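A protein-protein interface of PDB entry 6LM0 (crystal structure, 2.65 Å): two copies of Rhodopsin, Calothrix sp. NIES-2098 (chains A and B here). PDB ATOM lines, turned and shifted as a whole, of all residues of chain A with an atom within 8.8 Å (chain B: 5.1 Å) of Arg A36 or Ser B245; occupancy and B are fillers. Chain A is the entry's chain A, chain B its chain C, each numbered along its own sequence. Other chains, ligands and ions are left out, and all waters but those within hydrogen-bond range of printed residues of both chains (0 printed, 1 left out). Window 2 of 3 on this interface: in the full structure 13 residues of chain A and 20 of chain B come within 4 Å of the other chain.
No position is printed for both chains.
Of the 12 pairs that touch across the chains among the printed residues, none has its exchanged pair printed and touching as well.
Of the 10 printed residues of chain B, 6 touch a printed residue of chain A.
Hydrophobic or aromatic side chains of chain B that line the printed part of chain A: Tyr B242 and Met B243.
Of the 11 printed residues of chain A, 5 touch a printed residue of chain B.
Hydrophobic or aromatic side chains of chain A that line the printed part of chain B: Met A40.
Among the printed residues, Asp or Glu carboxylates within 4 Å of a Lys or Arg side-chain nitrogen of the other chain: Arg A37 with Glu B246.
The backbone carbonyl oxygen (O) of Ser B241 is in hydrogen-bond range of the side-chain hydroxyl (OG) of Ser B245.
NE of Arg B157 lies within hydrogen-bond range of O of Ala B153, at 2.8 Å.
The guanidinium group (NE) of Arg B100 lies close to the side-chain sulfur (SD) of Met B243 (3.7 Å).
NH1 of Arg B157 is in hydrogen-bond range of OG of Ser B241, at 2.8 Å.
NH2 of Arg A36 sits at hydrogen-bond distance from O of Ser B245, at 3.3 Å.
OE2 of Glu B246 is in salt-bridge range of NH2 of Arg A37, at 3.0 Å.
The guanidinium group (NH2) of Arg A36 lies within hydrogen-bond range of the backbone carbonyl oxygen (O) of Tyr B242 (3.1 Å).
The guanidinium group of Arg B100 sits at hydrogen-bond distance from the backbone carbonyl oxygen of Arg A37, 3.2 Å away.
The backbone carbonyl oxygen (O) of Met B243 lies close to the backbone carbonyl oxygen (O) of Arg A36 (3.2 Å).
The backbone carbonyl oxygen (O) of Arg A35 is in hydrogen-bond range of the guanidinium group (NH1) of Arg B100 (3.1 Å).
The guanidinium group of Arg A36 sits close to the guanidinium group of Arg B157 (3.5 Å).
Tyr B242 touches Arg A35 (OH to CD, 3.7 Å).
Arg B100 touches Arg A36 (NH1 to C, 3.97 Å).
Arg A37 touches Met B243 (C to CE, 3.6 Å).
Glu A38 touches Met B243.
Arg B100 touches Met A40 (NH2 to CE, 3.5 Å).
Arg A36 touches just these residues of chain B: Arg B100, Arg B157, Tyr B242, Met B243 and Ser B245.
Of chain A, only Arg A36 (3.3 Å) comes within 4 Å of Ser B245.
Met B243 touches just these residues of chain A: Arg A36 (3.2 Å), Arg A37 (3.6 Å) and Glu A38 (3.6 Å).
Of the printed residues of chain B, Glu A38 touches Met B243.
Of the printed residues of chain A, Glu B246 touches Arg A37 (3.0 Å).
Printed residues of chain B within 4 Å of Met A40: Arg B100 (3.5 Å).
Lys A30 touches none of the printed residues of chain B.
Ser A32 touches none of the printed residues of chain B.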
ATOM      1  N   LYS A  30     -18.462 -28.509  24.824  1.00  0.00           N
ATOM      2  CA  LYS A  30     -19.904 -28.292  24.768  1.00  0.00           C
ATOM      3  C   LYS A  30     -20.311 -27.510  23.524  1.00  0.00           C
ATOM      4  O   LYS A  30     -21.399 -27.735  22.986  1.00  0.00           O
ATOM      5  CB  LYS A  30     -20.377 -27.568  26.029  1.00  0.00           C
ATOM      6  CG  LYS A  30     -20.009 -28.272  27.325  1.00  0.00           C
ATOM      7  CD  LYS A  30     -21.227 -28.473  28.213  1.00  0.00           C
ATOM      8  CE  LYS A  30     -21.742 -29.900  28.131  1.00  0.00           C
ATOM      9  NZ  LYS A  30     -22.645 -30.231  29.268  1.00  0.00           N
ATOM     10  N   ALA A  31     -19.458 -26.597  23.053  1.00  0.00           N
ATOM     11  CA  ALA A  31     -19.798 -25.817  21.868  1.00  0.00           C
ATOM     12  C   ALA A  31     -19.813 -26.688  20.617  1.00  0.00           C
ATOM     13  O   ALA A  31     -20.676 -26.520  19.747  1.00  0.00           O
ATOM     14  CB  ALA A  31     -18.822 -24.653  21.699  1.00  0.00           C
ATOM     15  N   SER A  32     -18.867 -27.622  20.506  1.00  0.00           N
ATOM     16  CA  SER A  32     -18.825 -28.528  19.365  1.00  0.00           C
ATOM     17  C   SER A  32     -19.777 -29.706  19.509  1.00  0.00           C
ATOM     18  O   SER A  32     -19.962 -30.453  18.542  1.00  0.00           O
ATOM     19  CB  SER A  32     -17.396 -29.038  19.148  1.00  0.00           C
ATOM     20  OG  SER A  32     -16.955 -29.816  20.248  1.00  0.00           O
ATOM     21  N   ALA A  33     -20.380 -29.894  20.683  1.00  0.00           N
ATOM     22  CA  ALA A  33     -21.399 -30.918  20.867  1.00  0.00           C
ATOM     23  C   ALA A  33     -22.777 -30.473  20.397  1.00  0.00           C
ATOM     24  O   ALA A  33     -23.661 -31.320  20.228  1.00  0.00           O
ATOM     25  CB  ALA A  33     -21.471 -31.336  22.338  1.00  0.00           C
ATOM     26  N   MET A  34     -22.980 -29.175  20.181  1.00  0.00           N
ATOM     27  CA  MET A  34     -24.251 -28.633  19.720  1.00  0.00           C
ATOM     28  C   MET A  34     -24.036 -27.678  18.555  1.00  0.00           C
ATOM     29  O   MET A  34     -24.662 -26.619  18.472  1.00  0.00           O
ATOM     30  CB  MET A  34     -24.995 -27.936  20.857  1.00  0.00           C
ATOM     31  CG  MET A  34     -24.159 -26.932  21.632  1.00  0.00           C
ATOM     32  SD  MET A  34     -24.808 -26.623  23.287  1.00  0.00           S
ATOM     33  CE  MET A  34     -25.960 -25.294  22.957  1.00  0.00           C
ATOM     34  N   ARG A  35     -23.150 -28.047  17.625  1.00  0.00           N
ATOM     35  CA  ARG A  35     -22.853 -27.168  16.498  1.00  0.00           C
ATOM     36  C   ARG A  35     -24.052 -27.001  15.574  1.00  0.00           C
ATOM     37  O   ARG A  35     -24.156 -25.988  14.873  1.00  0.00           O
ATOM     38  CB  ARG A  35     -21.653 -27.701  15.716  1.00  0.00           C
ATOM     39  CG  ARG A  35     -21.708 -29.194  15.432  1.00  0.00           C
ATOM     40  CD  ARG A  35     -21.056 -29.528  14.098  1.00  0.00           C
ATOM     41  NE  ARG A  35     -19.634 -29.194  14.085  1.00  0.00           N
ATOM     42  CZ  ARG A  35     -18.662 -30.051  14.380  1.00  0.00           C
ATOM     43  NH1 ARG A  35     -18.953 -31.301  14.712  1.00  0.00           N
ATOM     44  NH2 ARG A  35     -17.395 -29.657  14.342  1.00  0.00           N
ATOM     45  N   ARG A  36     -24.963 -27.971  15.558  1.00  0.00           N
ATOM     46  CA  ARG A  36     -26.160 -27.908  14.729  1.00  0.00           C
ATOM     47  C   ARG A  36     -27.375 -27.374  15.476  1.00  0.00           C
ATOM     48  O   ARG A  36     -28.449 -27.259  14.876  1.00  0.00           O
ATOM     49  CB  ARG A  36     -26.483 -29.297  14.163  1.00  0.00           C
ATOM     50  CG  ARG A  36     -25.378 -29.914  13.321  1.00  0.00           C
ATOM     51  CD  ARG A  36     -25.894 -30.282  11.939  1.00  0.00           C
ATOM     52  NE  ARG A  36     -25.380 -31.565  11.469  1.00  0.00           N
ATOM     53  CZ  ARG A  36     -25.753 -32.145  10.333  1.00  0.00           C
ATOM     54  NH1 ARG A  36     -25.236 -33.314   9.982  1.00  0.00           N
ATOM     55  NH2 ARG A  36     -26.645 -31.557   9.547  1.00  0.00           N
ATOM     56  N   ARG A  37     -27.237 -27.041  16.755  1.00  0.00           N
ATOM     57  CA  ARG A  37     -28.368 -26.676  17.594  1.00  0.00           C
ATOM     58  C   ARG A  37     -28.439 -25.166  17.799  1.00  0.00           C
ATOM     59  O   ARG A  37     -27.494 -24.424  17.526  1.00  0.00           O
ATOM     60  CB  ARG A  37     -28.274 -27.387  18.948  1.00  0.00           C
ATOM     61  CG  ARG A  37     -28.108 -28.893  18.848  1.00  0.00           C
ATOM     62  CD  ARG A  37     -28.121 -29.537  20.222  1.00  0.00           C
ATOM     63  NE  ARG A  37     -27.326 -30.760  20.259  1.00  0.00           N
ATOM     64  CZ  ARG A  37     -27.835 -31.983  20.152  1.00  0.00           C
ATOM     65  NH1 ARG A  37     -29.143 -32.146  20.003  1.00  0.00           N
ATOM     66  NH2 ARG A  37     -27.039 -33.042  20.195  1.00  0.00           N
ATOM     67  N   GLU A  38     -29.594 -24.718  18.286  1.00  0.00           N
ATOM     68  CA  GLU A  38     -29.783 -23.335  18.693  1.00  0.00           C
ATOM     69  C   GLU A  38     -29.295 -23.147  20.124  1.00  0.00           C
ATOM     70  O   GLU A  38     -29.359 -24.064  20.948  1.00  0.00           O
ATOM     71  CB  GLU A  38     -31.253 -22.925  18.580  1.00  0.00           C
ATOM     72  CG  GLU A  38     -31.587 -22.151  17.312  1.00  0.00           C
ATOM     73  CD  GLU A  38     -31.057 -20.730  17.336  1.00  0.00           C
ATOM     74  OE1 GLU A  38     -30.805 -20.205  18.441  1.00  0.00           O
ATOM     75  OE2 GLU A  38     -30.891 -20.137  16.249  1.00  0.00           O
ATOM     76  N   GLY A  39     -28.810 -21.943  20.415  1.00  0.00           N
ATOM     77  CA  GLY A  39     -28.097 -21.696  21.648  1.00  0.00           C
ATOM     78  C   GLY A  39     -26.636 -22.083  21.609  1.00  0.00           C
ATOM     79  O   GLY A  39     -25.956 -21.988  22.638  1.00  0.00           O
ATOM     80  N   MET A  40     -26.136 -22.519  20.450  1.00  0.00           N
ATOM     81  CA  MET A  40     -24.736 -22.907  20.323  1.00  0.00           C
ATOM     82  C   MET A  40     -23.803 -21.721  20.526  1.00  0.00           C
ATOM     83  O   MET A  40     -22.654 -21.899  20.948  1.00  0.00           O
ATOM     84  CB  MET A  40     -24.513 -23.545  18.947  1.00  0.00           C
ATOM     85  CG  MET A  40     -23.063 -23.732  18.529  1.00  0.00           C
ATOM     86  SD  MET A  40     -22.412 -22.344  17.574  1.00  0.00           S
ATOM     87  CE  MET A  40     -23.851 -21.870  16.623  1.00  0.00           C
ATOM     88  N   ARG B 100     -24.271 -21.311   8.365  1.00  0.00           N
ATOM     89  CA  ARG B 100     -24.939 -20.328   9.202  1.00  0.00           C
ATOM     90  C   ARG B 100     -23.946 -19.248   9.624  1.00  0.00           C
ATOM     91  O   ARG B 100     -22.793 -19.557   9.950  1.00  0.00           O
ATOM     92  CB  ARG B 100     -25.563 -20.993  10.431  1.00  0.00           C
ATOM     93  CG  ARG B 100     -24.697 -22.053  11.086  1.00  0.00           C
ATOM     94  CD  ARG B 100     -25.489 -22.856  12.112  1.00  0.00           C
ATOM     95  NE  ARG B 100     -26.118 -22.000  13.114  1.00  0.00           N
ATOM     96  CZ  ARG B 100     -26.459 -22.404  14.335  1.00  0.00           C
ATOM     97  NH1 ARG B 100     -26.226 -23.655  14.711  1.00  0.00           N
ATOM     98  NH2 ARG B 100     -27.027 -21.557  15.181  1.00  0.00           N
ATOM     99  N   ALA B 153     -21.108 -30.134   5.117  1.00  0.00           N
ATOM    100  CA  ALA B 153     -22.450 -30.625   5.415  1.00  0.00           C
ATOM    101  C   ALA B 153     -23.525 -29.633   4.991  1.00  0.00           C
ATOM    102  O   ALA B 153     -24.638 -30.042   4.640  1.00  0.00           O
ATOM    103  CB  ALA B 153     -22.580 -30.939   6.904  1.00  0.00           C
ATOM    104  N   ARG B 157     -26.276 -30.016   0.941  1.00  0.00           N
ATOM    105  CA  ARG B 157     -27.723 -29.935   0.805  1.00  0.00           C
ATOM    106  C   ARG B 157     -28.168 -28.783  -0.084  1.00  0.00           C
ATOM    107  O   ARG B 157     -29.373 -28.532  -0.198  1.00  0.00           O
ATOM    108  CB  ARG B 157     -28.372 -29.803   2.186  1.00  0.00           C
ATOM    109  CG  ARG B 157     -28.206 -28.432   2.819  1.00  0.00           C
ATOM    110  CD  ARG B 157     -28.314 -28.511   4.330  1.00  0.00           C
ATOM    111  NE  ARG B 157     -27.365 -29.465   4.893  1.00  0.00           N
ATOM    112  CZ  ARG B 157     -27.710 -30.530   5.609  1.00  0.00           C
ATOM    113  NH1 ARG B 157     -28.991 -30.783   5.848  1.00  0.00           N
ATOM    114  NH2 ARG B 157     -26.777 -31.343   6.084  1.00  0.00           N
ATOM    115  N   SER B 241     -32.273 -26.532   7.016  1.00  0.00           N
ATOM    116  CA  SER B 241     -32.115 -27.964   6.787  1.00  0.00           C
ATOM    117  C   SER B 241     -30.914 -28.516   7.543  1.00  0.00           C
ATOM    118  O   SER B 241     -30.978 -29.618   8.100  1.00  0.00           O
ATOM    119  CB  SER B 241     -31.983 -28.245   5.291  1.00  0.00           C
ATOM    120  OG  SER B 241     -31.283 -29.456   5.065  1.00  0.00           O
ATOM    121  N   TYR B 242     -29.811 -27.764   7.573  1.00  0.00           N
ATOM    122  CA  TYR B 242     -28.626 -28.215   8.297  1.00  0.00           C
ATOM    123  C   TYR B 242     -28.888 -28.275   9.798  1.00  0.00           C
ATOM    124  O   TYR B 242     -28.471 -29.226  10.469  1.00  0.00           O
ATOM    125  CB  TYR B 242     -27.445 -27.293   7.986  1.00  0.00           C
ATOM    126  CG  TYR B 242     -26.223 -27.512   8.849  1.00  0.00           C
ATOM    127  CD1 TYR B 242     -25.284 -28.484   8.524  1.00  0.00           C
ATOM    128  CD2 TYR B 242     -25.997 -26.736   9.980  1.00  0.00           C
ATOM    129  CE1 TYR B 242     -24.163 -28.683   9.306  1.00  0.00           C
ATOM    130  CE2 TYR B 242     -24.878 -26.930  10.768  1.00  0.00           C
ATOM    131  CZ  TYR B 242     -23.965 -27.903  10.426  1.00  0.00           C
ATOM    132  OH  TYR B 242     -22.851 -28.098  11.210  1.00  0.00           O
ATOM    133  N   MET B 243     -29.585 -27.275  10.340  1.00  0.00           N
ATOM    134  CA  MET B 243     -29.840 -27.225  11.774  1.00  0.00           C
ATOM    135  C   MET B 243     -30.876 -28.242  12.233  1.00  0.00           C
ATOM    136  O   MET B 243     -30.987 -28.481  13.441  1.00  0.00           O
ATOM    137  CB  MET B 243     -30.295 -25.822  12.177  1.00  0.00           C
ATOM    138  CG  MET B 243     -29.192 -24.782  12.143  1.00  0.00           C
ATOM    139  SD  MET B 243     -29.603 -23.333  13.129  1.00  0.00           S
ATOM    140  CE  MET B 243     -29.961 -24.100  14.707  1.00  0.00           C
ATOM    141  N   GLN B 244     -31.631 -28.839  11.316  1.00  0.00           N
ATOM    142  CA  GLN B 244     -32.677 -29.787  11.671  1.00  0.00           C
ATOM    143  C   GLN B 244     -32.356 -31.217  11.264  1.00  0.00           C
ATOM    144  O   GLN B 244     -33.123 -32.126  11.595  1.00  0.00           O
ATOM    145  CB  GLN B 244     -34.011 -29.362  11.043  1.00  0.00           C
ATOM    146  CG  GLN B 244     -34.589 -28.075  11.610  1.00  0.00           C
ATOM    147  CD  GLN B 244     -35.847 -27.636  10.885  1.00  0.00           C
ATOM    148  OE1 GLN B 244     -36.748 -28.438  10.643  1.00  0.00           O
ATOM    149  NE2 GLN B 244     -35.912 -26.357  10.533  1.00  0.00           N
ATOM    150  N   SER B 245     -31.247 -31.445  10.560  1.00  0.00           N
ATOM    151  CA  SER B 245     -30.918 -32.786  10.094  1.00  0.00           C
ATOM    152  C   SER B 245     -29.753 -33.380  10.877  1.00  0.00           C
ATOM    153  O   SER B 245     -28.815 -33.921  10.283  1.00  0.00           O
ATOM    154  CB  SER B 245     -30.593 -32.769   8.599  1.00  0.00           C
ATOM    155  OG  SER B 245     -31.719 -32.370   7.836  1.00  0.00           O
ATOM    156  N   GLU B 246     -29.801 -33.289  12.206  1.00  0.00           N
ATOM    157  CA  GLU B 246     -28.783 -33.925  13.031  1.00  0.00           C
ATOM    158  C   GLU B 246     -28.959 -35.436  13.116  1.00  0.00           C
ATOM    159  O   GLU B 246     -28.075 -36.108  13.659  1.00  0.00           O
ATOM    160  CB  GLU B 246     -28.781 -33.322  14.439  1.00  0.00           C
ATOM    161  CG  GLU B 246     -27.411 -33.317  15.100  1.00  0.00           C
ATOM    162  CD  GLU B 246     -27.478 -33.083  16.596  1.00  0.00           C
ATOM    163  OE1 GLU B 246     -28.328 -32.281  17.038  1.00  0.00           O
ATOM    164  OE2 GLU B 246     -26.680 -33.703  17.331  1.00  0.00           O
ATOM    165  N   GLU B 247     -30.069 -35.962  12.592  1.00  0.00           N
ATOM    166  CA  GLU B 247     -30.379 -37.398  12.468  1.00  0.00           C
ATOM    167  C   GLU B 247     -29.541 -38.351  13.319  1.00  0.00           C
ATOM    168  O   GLU B 247     -29.089 -39.392  12.840  1.00  0.00           O
ATOM    169  CB  GLU B 247     -30.265 -37.817  10.998  1.00  0.00           C
ATOM    170  CG  GLU B 247     -29.108 -37.177  10.243  1.00  0.00           C
ATOM    171  CD  GLU B 247     -27.851 -38.021  10.277  1.00  0.00           C
ATOM    172  OE1 GLU B 247     -26.753 -37.451  10.448  1.00  0.00           O
ATOM    173  OE2 GLU B 247     -27.961 -39.256  10.130  1.00  0.00           O
